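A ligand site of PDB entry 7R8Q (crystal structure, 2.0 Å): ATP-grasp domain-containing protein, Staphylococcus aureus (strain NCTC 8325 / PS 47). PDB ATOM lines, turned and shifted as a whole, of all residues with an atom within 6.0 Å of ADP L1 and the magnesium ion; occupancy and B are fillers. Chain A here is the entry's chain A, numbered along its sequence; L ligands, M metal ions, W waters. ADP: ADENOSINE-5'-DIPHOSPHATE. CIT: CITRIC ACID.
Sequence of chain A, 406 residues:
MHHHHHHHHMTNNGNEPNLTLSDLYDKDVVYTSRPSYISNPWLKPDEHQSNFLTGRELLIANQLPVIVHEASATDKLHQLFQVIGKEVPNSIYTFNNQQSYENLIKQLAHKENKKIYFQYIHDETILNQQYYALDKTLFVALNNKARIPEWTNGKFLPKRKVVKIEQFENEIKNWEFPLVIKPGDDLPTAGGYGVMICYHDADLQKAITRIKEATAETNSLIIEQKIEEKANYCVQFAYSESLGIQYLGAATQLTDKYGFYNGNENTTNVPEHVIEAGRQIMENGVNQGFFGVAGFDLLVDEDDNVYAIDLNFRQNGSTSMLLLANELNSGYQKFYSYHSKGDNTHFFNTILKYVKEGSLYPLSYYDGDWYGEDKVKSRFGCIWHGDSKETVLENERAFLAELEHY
O3' of ADP L1 is in hydrogen-bond range of NE2 of Gln 253, 3.1 Å away. NZ of Lys 145 lies within salt-bridge range of O3B of ADP L1, 2.8 Å away. OG1 of Thr 255 lies within hydrogen-bond range of O2' of ADP L1 (2.9 Å). The backbone NH of Gly 192 is in hydrogen-bond range of an oxygen (O1B) of ADP L1 (2.5 Å). N6 of ADP L1 is in hydrogen-bond range of O of Gln 225, 2.9 Å away. The backbone NH (N) of Gly 191 sits at hydrogen-bond distance from an oxygen (O1B) of ADP L1 (3.3 Å). The backbone NH (N) of Ile 227 lies within hydrogen-bond range of a nitrogen (N1) of ADP L1, at 2.7 Å. O2' of ADP L1 lies within hydrogen-bond range of ND2 of Asn 232, at 3.1 Å. N6 of ADP L1 lies within hydrogen-bond range of OE1 of Glu 224, 2.7 Å away. The side-chain amino group (NZ) of Lys 182 is in salt-bridge range of an oxygen (O2A) of ADP L1 (2.7 Å).
The side-chain amino group (NZ) of Lys 182 lies within salt-bridge range of the side-chain carboxylate (OE1) of Glu 224 (3.3 Å). The side-chain amide nitrogen (NE2) of Gln 253 is in hydrogen-bond range of the side-chain amide oxygen (OD1) of Asn 232. NZ of Lys 182 lies within hydrogen-bond range of O of Ile 309, 3.1 Å away. NZ of Lys 226 lies within salt-bridge range of OE1 of Glu 229, 3.3 Å away. OD1 of Asp 297 sits at hydrogen-bond distance from ND2 of Asn 312 (3.3 Å). The backbone NH (N) of Val 180 is in hydrogen-bond range of the backbone carbonyl oxygen (O) of Glu 224 (2.7 Å). The side-chain amide nitrogen (NE2) of Gln 253 lies close to the side-chain carboxylate (OD2) of Asp 297. N of Gly 259 sits at hydrogen-bond distance from OD1 of Asp 256 (3.2 Å).
Residues that only touch ADP L1: Gly 259 (3.3 Å), Val 195 (3.4 Å), Ala 190 (3.4 Å), Lys 226 (3.4 Å), Leu 299 (3.4 Å), Ile 309 (3.6 Å), Ile 197 (3.7 Å), Val 180 (3.7 Å), Pro 158 (3.8 Å) and Glu 229 (3.9 Å). Hydrophobic or aromatic side chains that line ADP L1: Pro 158, Val 180, Val 195, Ile 197, Ile 227, Leu 299 and Ile 309. Within 4 Å of ADP L1: Lys 145, Pro 158, Val 180, Lys 182, Ala 190, Gly 191, Gly 192, Val 195, Ile 197, Glu 224, Gln 225, Lys 226, Ile 227, Glu 229, Asn 232, Gln 253, Thr 255, Gly 259, Asp 297, Leu 299, Ile 309 and Asp 310.
Of the 31 residues printed, 2 come within 4 Å of the magnesium ion. The nearest printed residue that does not touch the magnesium ion is Gln 253 (4.01 Å).
The magnesium ion is bound by O1A of ADP L1 (2.0 Å), O2B of ADP L1 (2.0 Å), OD2 of Asp 297 (2.0 Å), OD2 of Asp 310 (2.1 Å), O2 of CIT L2 (2.1 Å) and water W5 (2.1 Å). The magnesium ion has six donor atoms within binding distance.
Water W5 lies within hydrogen-bond range of the side-chain amide oxygen of Gln 253 and an oxygen (O3') of ADP L1. Water W6 lies within hydrogen-bond range of O3B of ADP L1 (2.5 Å), O of Thr 189 (2.8 Å), OD1 of Asn 312 (3.3 Å) and NH2 of Arg 314 (3.4 Å). Water W4 lies within hydrogen-bond range of the side-chain hydroxyl (OG1) of Thr 189 (2.7 Å), an oxygen (O1B) of ADP L1 (2.7 Å) and the backbone NH (N) of Gly 194 (2.8 Å). Water W2 bridges the side-chain carboxylate of Glu 229 and an oxygen (O2') of ADP L1. Water W1 lies within hydrogen-bond range of the backbone carbonyl oxygen of Gly 259 (2.7 Å) and the backbone NH of Gly 192 (3.4 Å). Water W3 lies within hydrogen-bond range of the backbone carbonyl oxygen of Asp 256, the side-chain hydroxyl of Thr 255 and an oxygen (O2') of ADP L1.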
ATOM      1  N   LYS A 145       8.737  22.978 -20.317  1.00  0.00           N
ATOM      2  CA  LYS A 145       8.370  22.611 -21.683  1.00  0.00           C
ATOM      3  C   LYS A 145       8.885  23.624 -22.704  1.00  0.00           C
ATOM      4  O   LYS A 145       9.179  23.256 -23.841  1.00  0.00           O
ATOM      5  CB  LYS A 145       6.856  22.467 -21.811  1.00  0.00           C
ATOM      6  CG  LYS A 145       6.336  21.122 -21.340  1.00  0.00           C
ATOM      7  CD  LYS A 145       4.851  20.985 -21.590  1.00  0.00           C
ATOM      8  CE  LYS A 145       4.299  19.773 -20.868  1.00  0.00           C
ATOM      9  NZ  LYS A 145       2.841  19.621 -21.078  1.00  0.00           N
ATOM     10  N   PRO A 158       7.939  19.461 -32.689  1.00  0.00           N
ATOM     11  CA  PRO A 158       6.979  19.942 -33.684  1.00  0.00           C
ATOM     12  C   PRO A 158       7.267  21.393 -34.028  1.00  0.00           C
ATOM     13  O   PRO A 158       7.993  22.093 -33.322  1.00  0.00           O
ATOM     14  CB  PRO A 158       5.625  19.785 -32.982  1.00  0.00           C
ATOM     15  CG  PRO A 158       5.866  18.775 -31.881  1.00  0.00           C
ATOM     16  CD  PRO A 158       7.276  19.053 -31.438  1.00  0.00           C
ATOM     17  N   VAL A 180      -1.623  22.993 -30.487  1.00  0.00           N
ATOM     18  CA  VAL A 180      -1.581  22.867 -29.030  1.00  0.00           C
ATOM     19  C   VAL A 180      -1.001  24.154 -28.451  1.00  0.00           C
ATOM     20  O   VAL A 180      -0.028  24.704 -28.975  1.00  0.00           O
ATOM     21  CB  VAL A 180      -0.740  21.654 -28.569  1.00  0.00           C
ATOM     22  CG1 VAL A 180      -0.957  21.408 -27.099  1.00  0.00           C
ATOM     23  CG2 VAL A 180      -1.069  20.412 -29.394  1.00  0.00           C
ATOM     24  N   LYS A 182       0.468  25.620 -24.779  1.00  0.00           N
ATOM     25  CA  LYS A 182       0.962  25.215 -23.467  1.00  0.00           C
ATOM     26  C   LYS A 182       1.590  26.410 -22.762  1.00  0.00           C
ATOM     27  O   LYS A 182       2.180  27.272 -23.420  1.00  0.00           O
ATOM     28  CB  LYS A 182       1.979  24.081 -23.575  1.00  0.00           C
ATOM     29  CG  LYS A 182       1.501  22.891 -24.413  1.00  0.00           C
ATOM     30  CD  LYS A 182       2.560  21.791 -24.464  1.00  0.00           C
ATOM     31  CE  LYS A 182       2.168  20.721 -25.482  1.00  0.00           C
ATOM     32  NZ  LYS A 182       3.127  19.585 -25.525  1.00  0.00           N
ATOM     33  N   THR A 189       3.457  21.248 -14.106  1.00  0.00           N
ATOM     34  CA  THR A 189       2.266  20.756 -14.798  1.00  0.00           C
ATOM     35  C   THR A 189       2.488  19.285 -15.105  1.00  0.00           C
ATOM     36  O   THR A 189       3.622  18.803 -15.163  1.00  0.00           O
ATOM     37  CB  THR A 189       1.987  21.560 -16.067  1.00  0.00           C
ATOM     38  OG1 THR A 189       0.685  21.204 -16.570  1.00  0.00           O
ATOM     39  CG2 THR A 189       3.028  21.263 -17.138  1.00  0.00           C
ATOM     40  N   ALA A 190       1.382  18.573 -15.305  1.00  0.00           N
ATOM     41  CA  ALA A 190       1.393  17.127 -15.546  1.00  0.00           C
ATOM     42  C   ALA A 190      -0.046  16.687 -15.793  1.00  0.00           C
ATOM     43  O   ALA A 190      -0.994  17.440 -15.595  1.00  0.00           O
ATOM     44  CB  ALA A 190       2.016  16.365 -14.371  1.00  0.00           C
ATOM     45  N   GLY A 191      -0.173  15.436 -16.255  1.00  0.00           N
ATOM     46  CA  GLY A 191      -1.457  14.774 -16.395  1.00  0.00           C
ATOM     47  C   GLY A 191      -2.417  15.374 -17.398  1.00  0.00           C
ATOM     48  O   GLY A 191      -3.588  14.976 -17.432  1.00  0.00           O
ATOM     49  N   GLY A 192      -1.977  16.327 -18.217  1.00  0.00           N
ATOM     50  CA  GLY A 192      -2.882  16.989 -19.122  1.00  0.00           C
ATOM     51  C   GLY A 192      -3.626  18.148 -18.528  1.00  0.00           C
ATOM     52  O   GLY A 192      -4.539  18.685 -19.168  1.00  0.00           O
ATOM     53  N   TYR A 193      -3.278  18.568 -17.305  1.00  0.00           N
ATOM     54  CA  TYR A 193      -3.964  19.688 -16.661  1.00  0.00           C
ATOM     55  C   TYR A 193      -3.545  21.037 -17.215  1.00  0.00           C
ATOM     56  O   TYR A 193      -4.241  22.028 -16.969  1.00  0.00           O
ATOM     57  CB  TYR A 193      -3.721  19.638 -15.153  1.00  0.00           C
ATOM     58  CG  TYR A 193      -4.514  18.566 -14.449  1.00  0.00           C
ATOM     59  CD1 TYR A 193      -5.826  18.809 -14.043  1.00  0.00           C
ATOM     60  CD2 TYR A 193      -3.960  17.324 -14.171  1.00  0.00           C
ATOM     61  CE1 TYR A 193      -6.565  17.839 -13.390  1.00  0.00           C
ATOM     62  CE2 TYR A 193      -4.694  16.341 -13.523  1.00  0.00           C
ATOM     63  CZ  TYR A 193      -5.996  16.601 -13.128  1.00  0.00           C
ATOM     64  OH  TYR A 193      -6.727  15.635 -12.478  1.00  0.00           O
ATOM     65  N   GLY A 194      -2.435  21.117 -17.952  1.00  0.00           N
ATOM     66  CA  GLY A 194      -1.988  22.378 -18.506  1.00  0.00           C
ATOM     67  C   GLY A 194      -1.671  22.306 -19.982  1.00  0.00           C
ATOM     68  O   GLY A 194      -0.611  22.777 -20.414  1.00  0.00           O
ATOM     69  N   VAL A 195      -2.571  21.717 -20.766  1.00  0.00           N
ATOM     70  CA  VAL A 195      -2.407  21.592 -22.208  1.00  0.00           C
ATOM     71  C   VAL A 195      -3.753  21.879 -22.870  1.00  0.00           C
ATOM     72  O   VAL A 195      -4.791  21.565 -22.286  1.00  0.00           O
ATOM     73  CB  VAL A 195      -1.901  20.185 -22.604  1.00  0.00           C
ATOM     74  CG1 VAL A 195      -2.199  19.890 -24.053  1.00  0.00           C
ATOM     75  CG2 VAL A 195      -0.398  20.062 -22.327  1.00  0.00           C
ATOM     76  N   ILE A 197      -5.395  21.597 -26.402  1.00  0.00           N
ATOM     77  CA  ILE A 197      -5.375  21.114 -27.779  1.00  0.00           C
ATOM     78  C   ILE A 197      -6.608  21.669 -28.499  1.00  0.00           C
ATOM     79  O   ILE A 197      -7.736  21.496 -28.042  1.00  0.00           O
ATOM     80  CB  ILE A 197      -5.358  19.571 -27.829  1.00  0.00           C
ATOM     81  CG1 ILE A 197      -4.187  19.028 -27.007  1.00  0.00           C
ATOM     82  CG2 ILE A 197      -5.265  19.093 -29.263  1.00  0.00           C
ATOM     83  CD1 ILE A 197      -4.019  17.528 -27.109  1.00  0.00           C
ATOM     84  N   GLU A 224       2.218  25.139 -30.696  1.00  0.00           N
ATOM     85  CA  GLU A 224       2.832  23.932 -31.227  1.00  0.00           C
ATOM     86  C   GLU A 224       1.880  23.266 -32.204  1.00  0.00           C
ATOM     87  O   GLU A 224       0.670  23.198 -31.935  1.00  0.00           O
ATOM     88  CB  GLU A 224       3.183  22.980 -30.078  1.00  0.00           C
ATOM     89  CG  GLU A 224       4.274  21.979 -30.348  1.00  0.00           C
ATOM     90  CD  GLU A 224       4.637  21.208 -29.095  1.00  0.00           C
ATOM     91  OE1 GLU A 224       3.804  20.398 -28.636  1.00  0.00           O
ATOM     92  OE2 GLU A 224       5.744  21.437 -28.558  1.00  0.00           O
ATOM     93  N   GLN A 225       2.407  22.790 -33.328  1.00  0.00           N
ATOM     94  CA  GLN A 225       1.561  22.028 -34.251  1.00  0.00           C
ATOM     95  C   GLN A 225       1.155  20.714 -33.591  1.00  0.00           C
ATOM     96  O   GLN A 225       1.955  20.069 -32.902  1.00  0.00           O
ATOM     97  CB  GLN A 225       2.288  21.754 -35.578  1.00  0.00           C
ATOM     98  CG  GLN A 225       3.286  20.592 -35.541  1.00  0.00           C
ATOM     99  CD  GLN A 225       3.812  20.205 -36.910  1.00  0.00           C
ATOM    100  OE1 GLN A 225       5.023  20.028 -37.089  1.00  0.00           O
ATOM    101  NE2 GLN A 225       2.923  20.041 -37.886  1.00  0.00           N
ATOM    102  N   LYS A 226      -0.112  20.347 -33.770  1.00  0.00           N
ATOM    103  CA  LYS A 226      -0.609  19.087 -33.245  1.00  0.00           C
ATOM    104  C   LYS A 226      -0.190  17.971 -34.208  1.00  0.00           C
ATOM    105  O   LYS A 226      -0.617  17.947 -35.357  1.00  0.00           O
ATOM    106  CB  LYS A 226      -2.131  19.132 -33.076  1.00  0.00           C
ATOM    107  CG  LYS A 226      -2.819  17.780 -32.997  1.00  0.00           C
ATOM    108  CD  LYS A 226      -2.789  17.191 -31.603  1.00  0.00           C
ATOM    109  CE  LYS A 226      -3.659  15.947 -31.508  1.00  0.00           C
ATOM    110  NZ  LYS A 226      -3.257  14.855 -32.448  1.00  0.00           N
ATOM    111  N   ILE A 227       0.671  17.071 -33.729  1.00  0.00           N
ATOM    112  CA  ILE A 227       1.182  15.984 -34.556  1.00  0.00           C
ATOM    113  C   ILE A 227       0.105  14.918 -34.688  1.00  0.00           C
ATOM    114  O   ILE A 227      -0.535  14.526 -33.701  1.00  0.00           O
ATOM    115  CB  ILE A 227       2.476  15.411 -33.949  1.00  0.00           C
ATOM    116  CG1 ILE A 227       3.589  16.448 -34.000  1.00  0.00           C
ATOM    117  CG2 ILE A 227       2.898  14.147 -34.680  1.00  0.00           C
ATOM    118  CD1 ILE A 227       3.895  16.953 -35.394  1.00  0.00           C
ATOM    119  N   GLU A 228      -0.103  14.431 -35.913  1.00  0.00           N
ATOM    120  CA  GLU A 228      -1.034  13.341 -36.172  1.00  0.00           C
ATOM    121  C   GLU A 228      -0.314  12.027 -35.896  1.00  0.00           C
ATOM    122  O   GLU A 228       0.153  11.333 -36.800  1.00  0.00           O
ATOM    123  CB  GLU A 228      -1.559  13.421 -37.599  1.00  0.00           C
ATOM    124  CG  GLU A 228      -2.849  12.648 -37.848  1.00  0.00           C
ATOM    125  CD  GLU A 228      -3.335  12.781 -39.285  1.00  0.00           C
ATOM    126  OE1 GLU A 228      -4.112  11.913 -39.742  1.00  0.00           O
ATOM    127  OE2 GLU A 228      -2.932  13.761 -39.954  1.00  0.00           O
ATOM    128  N   GLU A 229      -0.232  11.687 -34.611  1.00  0.00           N
ATOM    129  CA  GLU A 229       0.652  10.600 -34.191  1.00  0.00           C
ATOM    130  C   GLU A 229       0.033   9.243 -34.473  1.00  0.00           C
ATOM    131  O   GLU A 229      -1.192   9.061 -34.392  1.00  0.00           O
ATOM    132  CB  GLU A 229       0.987  10.737 -32.704  1.00  0.00           C
ATOM    133  CG  GLU A 229      -0.088  10.248 -31.733  1.00  0.00           C
ATOM    134  CD  GLU A 229      -1.109  11.312 -31.390  1.00  0.00           C
ATOM    135  OE1 GLU A 229      -1.081  12.400 -31.999  1.00  0.00           O
ATOM    136  OE2 GLU A 229      -1.953  11.067 -30.498  1.00  0.00           O
ATOM    137  N   ASN A 232       2.269   6.871 -29.318  1.00  0.00           N
ATOM    138  CA  ASN A 232       2.530   7.849 -28.270  1.00  0.00           C
ATOM    139  C   ASN A 232       3.226   7.096 -27.142  1.00  0.00           C
ATOM    140  O   ASN A 232       2.563   6.460 -26.315  1.00  0.00           O
ATOM    141  CB  ASN A 232       1.242   8.504 -27.786  1.00  0.00           C
ATOM    142  CG  ASN A 232       1.477   9.621 -26.778  1.00  0.00           C
ATOM    143  OD1 ASN A 232       2.545   9.707 -26.157  1.00  0.00           O
ATOM    144  ND2 ASN A 232       0.485  10.490 -26.606  1.00  0.00           N
ATOM    145  N   GLN A 253       1.003   5.795 -24.136  1.00  0.00           N
ATOM    146  CA  GLN A 253       0.174   6.675 -23.320  1.00  0.00           C
ATOM    147  C   GLN A 253      -1.286   6.519 -23.711  1.00  0.00           C
ATOM    148  O   GLN A 253      -1.616   6.433 -24.893  1.00  0.00           O
ATOM    149  CB  GLN A 253       0.589   8.145 -23.493  1.00  0.00           C
ATOM    150  CG  GLN A 253       1.992   8.462 -23.013  1.00  0.00           C
ATOM    151  CD  GLN A 253       2.174   9.940 -22.741  1.00  0.00           C
ATOM    152  OE1 GLN A 253       1.911  10.405 -21.627  1.00  0.00           O
ATOM    153  NE2 GLN A 253       2.590  10.687 -23.753  1.00  0.00           N
ATOM    154  N   THR A 255      -4.130   8.830 -23.526  1.00  0.00           N
ATOM    155  CA  THR A 255      -4.547  10.219 -23.348  1.00  0.00           C
ATOM    156  C   THR A 255      -5.733  10.486 -24.268  1.00  0.00           C
ATOM    157  O   THR A 255      -5.791   9.955 -25.380  1.00  0.00           O
ATOM    158  CB  THR A 255      -3.402  11.200 -23.659  1.00  0.00           C
ATOM    159  OG1 THR A 255      -2.911  10.974 -24.976  1.00  0.00           O
ATOM    160  CG2 THR A 255      -2.258  11.021 -22.657  1.00  0.00           C
ATOM    161  N   ASP A 256      -6.676  11.299 -23.806  1.00  0.00           N
ATOM    162  CA  ASP A 256      -7.876  11.519 -24.595  1.00  0.00           C
ATOM    163  C   ASP A 256      -7.597  12.580 -25.664  1.00  0.00           C
ATOM    164  O   ASP A 256      -6.445  13.000 -25.870  1.00  0.00           O
ATOM    165  CB  ASP A 256      -9.076  11.851 -23.699  1.00  0.00           C
ATOM    166  CG  ASP A 256      -9.004  13.234 -23.040  1.00  0.00           C
ATOM    167  OD1 ASP A 256      -8.170  14.085 -23.441  1.00  0.00           O
ATOM    168  OD2 ASP A 256      -9.797  13.471 -22.112  1.00  0.00           O
ATOM    169  N   TYR A 258      -8.012  15.667 -25.777  1.00  0.00           N
ATOM    170  CA  TYR A 258      -7.466  16.928 -25.284  1.00  0.00           C
ATOM    171  C   TYR A 258      -6.191  16.727 -24.467  1.00  0.00           C
ATOM    172  O   TYR A 258      -5.776  17.653 -23.762  1.00  0.00           O
ATOM    173  CB  TYR A 258      -8.523  17.659 -24.453  1.00  0.00           C
ATOM    174  CG  TYR A 258      -9.750  18.011 -25.267  1.00  0.00           C
ATOM    175  CD1 TYR A 258      -9.617  18.626 -26.509  1.00  0.00           C
ATOM    176  CD2 TYR A 258     -11.029  17.718 -24.807  1.00  0.00           C
ATOM    177  CE1 TYR A 258     -10.726  18.950 -27.262  1.00  0.00           C
ATOM    178  CE2 TYR A 258     -12.139  18.037 -25.569  1.00  0.00           C
ATOM    179  CZ  TYR A 258     -11.986  18.647 -26.799  1.00  0.00           C
ATOM    180  OH  TYR A 258     -13.074  18.969 -27.565  1.00  0.00           O
ATOM    181  N   GLY A 259      -5.584  15.552 -24.543  1.00  0.00           N
ATOM    182  CA  GLY A 259      -4.334  15.287 -23.872  1.00  0.00           C
ATOM    183  C   GLY A 259      -4.442  14.888 -22.420  1.00  0.00           C
ATOM    184  O   GLY A 259      -3.408  14.705 -21.760  1.00  0.00           O
ATOM    185  N   PHE A 260      -5.656  14.752 -21.883  1.00  0.00           N
ATOM    186  CA  PHE A 260      -5.825  14.375 -20.482  1.00  0.00           C
ATOM    187  C   PHE A 260      -5.317  12.958 -20.263  1.00  0.00           C
ATOM    188  O   PHE A 260      -5.653  12.033 -21.012  1.00  0.00           O
ATOM    189  CB  PHE A 260      -7.296  14.493 -20.071  1.00  0.00           C
ATOM    190  CG  PHE A 260      -7.516  14.346 -18.586  1.00  0.00           C
ATOM    191  CD1 PHE A 260      -7.945  13.143 -18.055  1.00  0.00           C
ATOM    192  CD2 PHE A 260      -7.263  15.405 -17.731  1.00  0.00           C
ATOM    193  CE1 PHE A 260      -8.136  13.004 -16.692  1.00  0.00           C
ATOM    194  CE2 PHE A 260      -7.459  15.277 -16.364  1.00  0.00           C
ATOM    195  CZ  PHE A 260      -7.896  14.072 -15.853  1.00  0.00           C
ATOM    196  N   ASP A 297       7.942  11.786 -23.424  1.00  0.00           N
ATOM    197  CA  ASP A 297       6.823  11.543 -24.320  1.00  0.00           C
ATOM    198  C   ASP A 297       7.312  11.707 -25.762  1.00  0.00           C
ATOM    199  O   ASP A 297       7.597  12.826 -26.197  1.00  0.00           O
ATOM    200  CB  ASP A 297       5.669  12.508 -24.046  1.00  0.00           C
ATOM    201  CG  ASP A 297       5.016  12.276 -22.699  1.00  0.00           C
ATOM    202  OD1 ASP A 297       5.567  11.483 -21.901  1.00  0.00           O
ATOM    203  OD2 ASP A 297       3.956  12.884 -22.442  1.00  0.00           O
ATOM    204  N   LEU A 299       6.237  10.995 -29.609  1.00  0.00           N
ATOM    205  CA  LEU A 299       5.256  10.644 -30.620  1.00  0.00           C
ATOM    206  C   LEU A 299       5.956  10.138 -31.872  1.00  0.00           C
ATOM    207  O   LEU A 299       7.106  10.507 -32.153  1.00  0.00           O
ATOM    208  CB  LEU A 299       4.378  11.847 -30.980  1.00  0.00           C
ATOM    209  CG  LEU A 299       3.794  12.680 -29.842  1.00  0.00           C
ATOM    210  CD1 LEU A 299       2.876  13.741 -30.405  1.00  0.00           C
ATOM    211  CD2 LEU A 299       3.066  11.797 -28.847  1.00  0.00           C
ATOM    212  N   ILE A 309       7.525  15.887 -27.297  1.00  0.00           N
ATOM    213  CA  ILE A 309       6.541  16.916 -26.974  1.00  0.00           C
ATOM    214  C   ILE A 309       6.527  17.276 -25.494  1.00  0.00           C
ATOM    215  O   ILE A 309       5.960  18.307 -25.124  1.00  0.00           O
ATOM    216  CB  ILE A 309       5.129  16.473 -27.417  1.00  0.00           C
ATOM    217  CG1 ILE A 309       4.760  15.161 -26.727  1.00  0.00           C
ATOM    218  CG2 ILE A 309       5.081  16.328 -28.917  1.00  0.00           C
ATOM    219  CD1 ILE A 309       3.272  14.876 -26.676  1.00  0.00           C
ATOM    220  N   ASP A 310       7.137  16.448 -24.637  1.00  0.00           N
ATOM    221  CA  ASP A 310       7.037  16.613 -23.190  1.00  0.00           C
ATOM    222  C   ASP A 310       8.144  15.799 -22.543  1.00  0.00           C
ATOM    223  O   ASP A 310       8.190  14.581 -22.708  1.00  0.00           O
ATOM    224  CB  ASP A 310       5.653  16.170 -22.694  1.00  0.00           C
ATOM    225  CG  ASP A 310       5.556  16.147 -21.187  1.00  0.00           C
ATOM    226  OD1 ASP A 310       6.250  16.950 -20.524  1.00  0.00           O
ATOM    227  OD2 ASP A 310       4.797  15.310 -20.652  1.00  0.00           O
ATOM    228  N   ASN A 312       9.712  14.585 -19.008  1.00  0.00           N
ATOM    229  CA  ASN A 312       9.413  14.400 -17.586  1.00  0.00           C
ATOM    230  C   ASN A 312      10.671  13.908 -16.893  1.00  0.00           C
ATOM    231  O   ASN A 312      10.902  12.713 -16.746  1.00  0.00           O
ATOM    232  CB  ASN A 312       8.254  13.427 -17.382  1.00  0.00           C
ATOM    233  CG  ASN A 312       7.029  13.827 -18.154  1.00  0.00           C
ATOM    234  OD1 ASN A 312       6.417  14.852 -17.867  1.00  0.00           O
ATOM    235  ND2 ASN A 312       6.673  13.038 -19.160  1.00  0.00           N
ATOM    236  N   ARG A 314      11.677  13.148 -14.047  1.00  0.00           N
ATOM    237  CA  ARG A 314      11.123  12.667 -12.789  1.00  0.00           C
ATOM    238  C   ARG A 314      10.425  11.356 -13.100  1.00  0.00           C
ATOM    239  O   ARG A 314      10.237  10.983 -14.264  1.00  0.00           O
ATOM    240  CB  ARG A 314      10.126  13.657 -12.178  1.00  0.00           C
ATOM    241  CG  ARG A 314       9.098  14.163 -13.179  1.00  0.00           C
ATOM    242  CD  ARG A 314       7.927  14.822 -12.480  1.00  0.00           C
ATOM    243  NE  ARG A 314       6.985  15.441 -13.415  1.00  0.00           N
ATOM    244  CZ  ARG A 314       6.043  14.777 -14.084  1.00  0.00           C
ATOM    245  NH1 ARG A 314       5.923  13.468 -13.928  1.00  0.00           N
ATOM    246  NH2 ARG A 314       5.235  15.424 -14.899  1.00  0.00           N
HETATM  247  PB  ADP L   1       1.628  16.800 -19.769  1.00  0.00           P
HETATM  248  O1B ADP L   1       0.273  17.034 -19.135  1.00  0.00           O
HETATM  249  O2B ADP L   1       1.946  15.336 -19.964  1.00  0.00           O
HETATM  250  O3B ADP L   1       2.727  17.578 -19.099  1.00  0.00           O
HETATM  251  PA  ADP L   1       1.919  16.900 -22.660  1.00  0.00           P
HETATM  252  O1A ADP L   1       2.443  15.498 -22.497  1.00  0.00           O
HETATM  253  O2A ADP L   1       2.735  17.943 -23.408  1.00  0.00           O
HETATM  254  O3A ADP L   1       1.504  17.507 -21.219  1.00  0.00           O
HETATM  255  O5' ADP L   1       0.494  16.790 -23.391  1.00  0.00           O
HETATM  256  C5' ADP L   1      -0.376  15.740 -23.002  1.00  0.00           C
HETATM  257  C4' ADP L   1      -0.869  14.949 -24.211  1.00  0.00           C
HETATM  258  O4' ADP L   1      -1.356  15.825 -25.233  1.00  0.00           O
HETATM  259  C3' ADP L   1       0.197  14.104 -24.864  1.00  0.00           C
HETATM  260  O3' ADP L   1       0.337  12.830 -24.238  1.00  0.00           O
HETATM  261  C2' ADP L   1      -0.312  13.993 -26.288  1.00  0.00           C
HETATM  262  O2' ADP L   1      -1.295  12.965 -26.382  1.00  0.00           O
HETATM  263  C1' ADP L   1      -1.033  15.302 -26.516  1.00  0.00           C
HETATM  264  N9  ADP L   1      -0.136  16.274 -27.176  1.00  0.00           N
HETATM  265  C8  ADP L   1       0.535  17.269 -26.559  1.00  0.00           C
HETATM  266  N7  ADP L   1       1.266  18.000 -27.446  1.00  0.00           N
HETATM  267  C5  ADP L   1       1.068  17.457 -28.663  1.00  0.00           C
HETATM  268  C6  ADP L   1       1.523  17.746 -30.045  1.00  0.00           C
HETATM  269  N6  ADP L   1       2.375  18.774 -30.305  1.00  0.00           N
HETATM  270  N1  ADP L   1       1.071  16.943 -31.033  1.00  0.00           N
HETATM  271  C2  ADP L   1       0.234  15.919 -30.788  1.00  0.00           C
HETATM  272  N3  ADP L   1      -0.225  15.607 -29.565  1.00  0.00           N
HETATM  273  C4  ADP L   1       0.141  16.333 -28.479  1.00  0.00           C
HETATM  274  C1  CIT L   2       3.418  11.721 -19.151  1.00  0.00           C
HETATM  275  O1  CIT L   2       4.245  10.896 -19.584  1.00  0.00           O
HETATM  276  O2  CIT L   2       3.509  12.911 -19.536  1.00  0.00           O
HETATM  277  C2  CIT L   2       2.343  11.269 -18.188  1.00  0.00           C
HETATM  278  C3  CIT L   2       1.874  12.385 -17.254  1.00  0.00           C
HETATM  279  O7  CIT L   2       1.083  13.326 -18.029  1.00  0.00           O
HETATM  280  C4  CIT L   2       0.967  11.869 -16.136  1.00  0.00           C
HETATM  281  C5  CIT L   2       1.685  10.994 -15.126  1.00  0.00           C
HETATM  282  O3  CIT L   2       1.701  11.329 -13.923  1.00  0.00           O
HETATM  283  O4  CIT L   2       2.252   9.929 -15.454  1.00  0.00           O
HETATM  284  C6  CIT L   2       3.058  13.118 -16.650  1.00  0.00           C
HETATM  285  O5  CIT L   2       4.052  12.484 -16.240  1.00  0.00           O
HETATM  286  O6  CIT L   2       3.052  14.362 -16.584  1.00  0.00           O
HETATM  287 MG    MG M   1       3.108  14.204 -21.157  1.00  0.00          MG
HETATM  288  O   HOH W   1      -1.107  14.003 -20.508  1.00  0.00           O
HETATM  289  O   HOH W   2      -2.060  13.265 -29.078  1.00  0.00           O
HETATM  290  O   HOH W   3      -4.321  12.282 -27.683  1.00  0.00           O
HETATM  291  O   HOH W   4      -0.173  19.649 -18.545  1.00  0.00           O
HETATM  292  O   HOH W   5       1.382  13.096 -21.691  1.00  0.00           O
HETATM  293  O   HOH W   6       4.591  17.543 -17.426  1.00  0.00           O
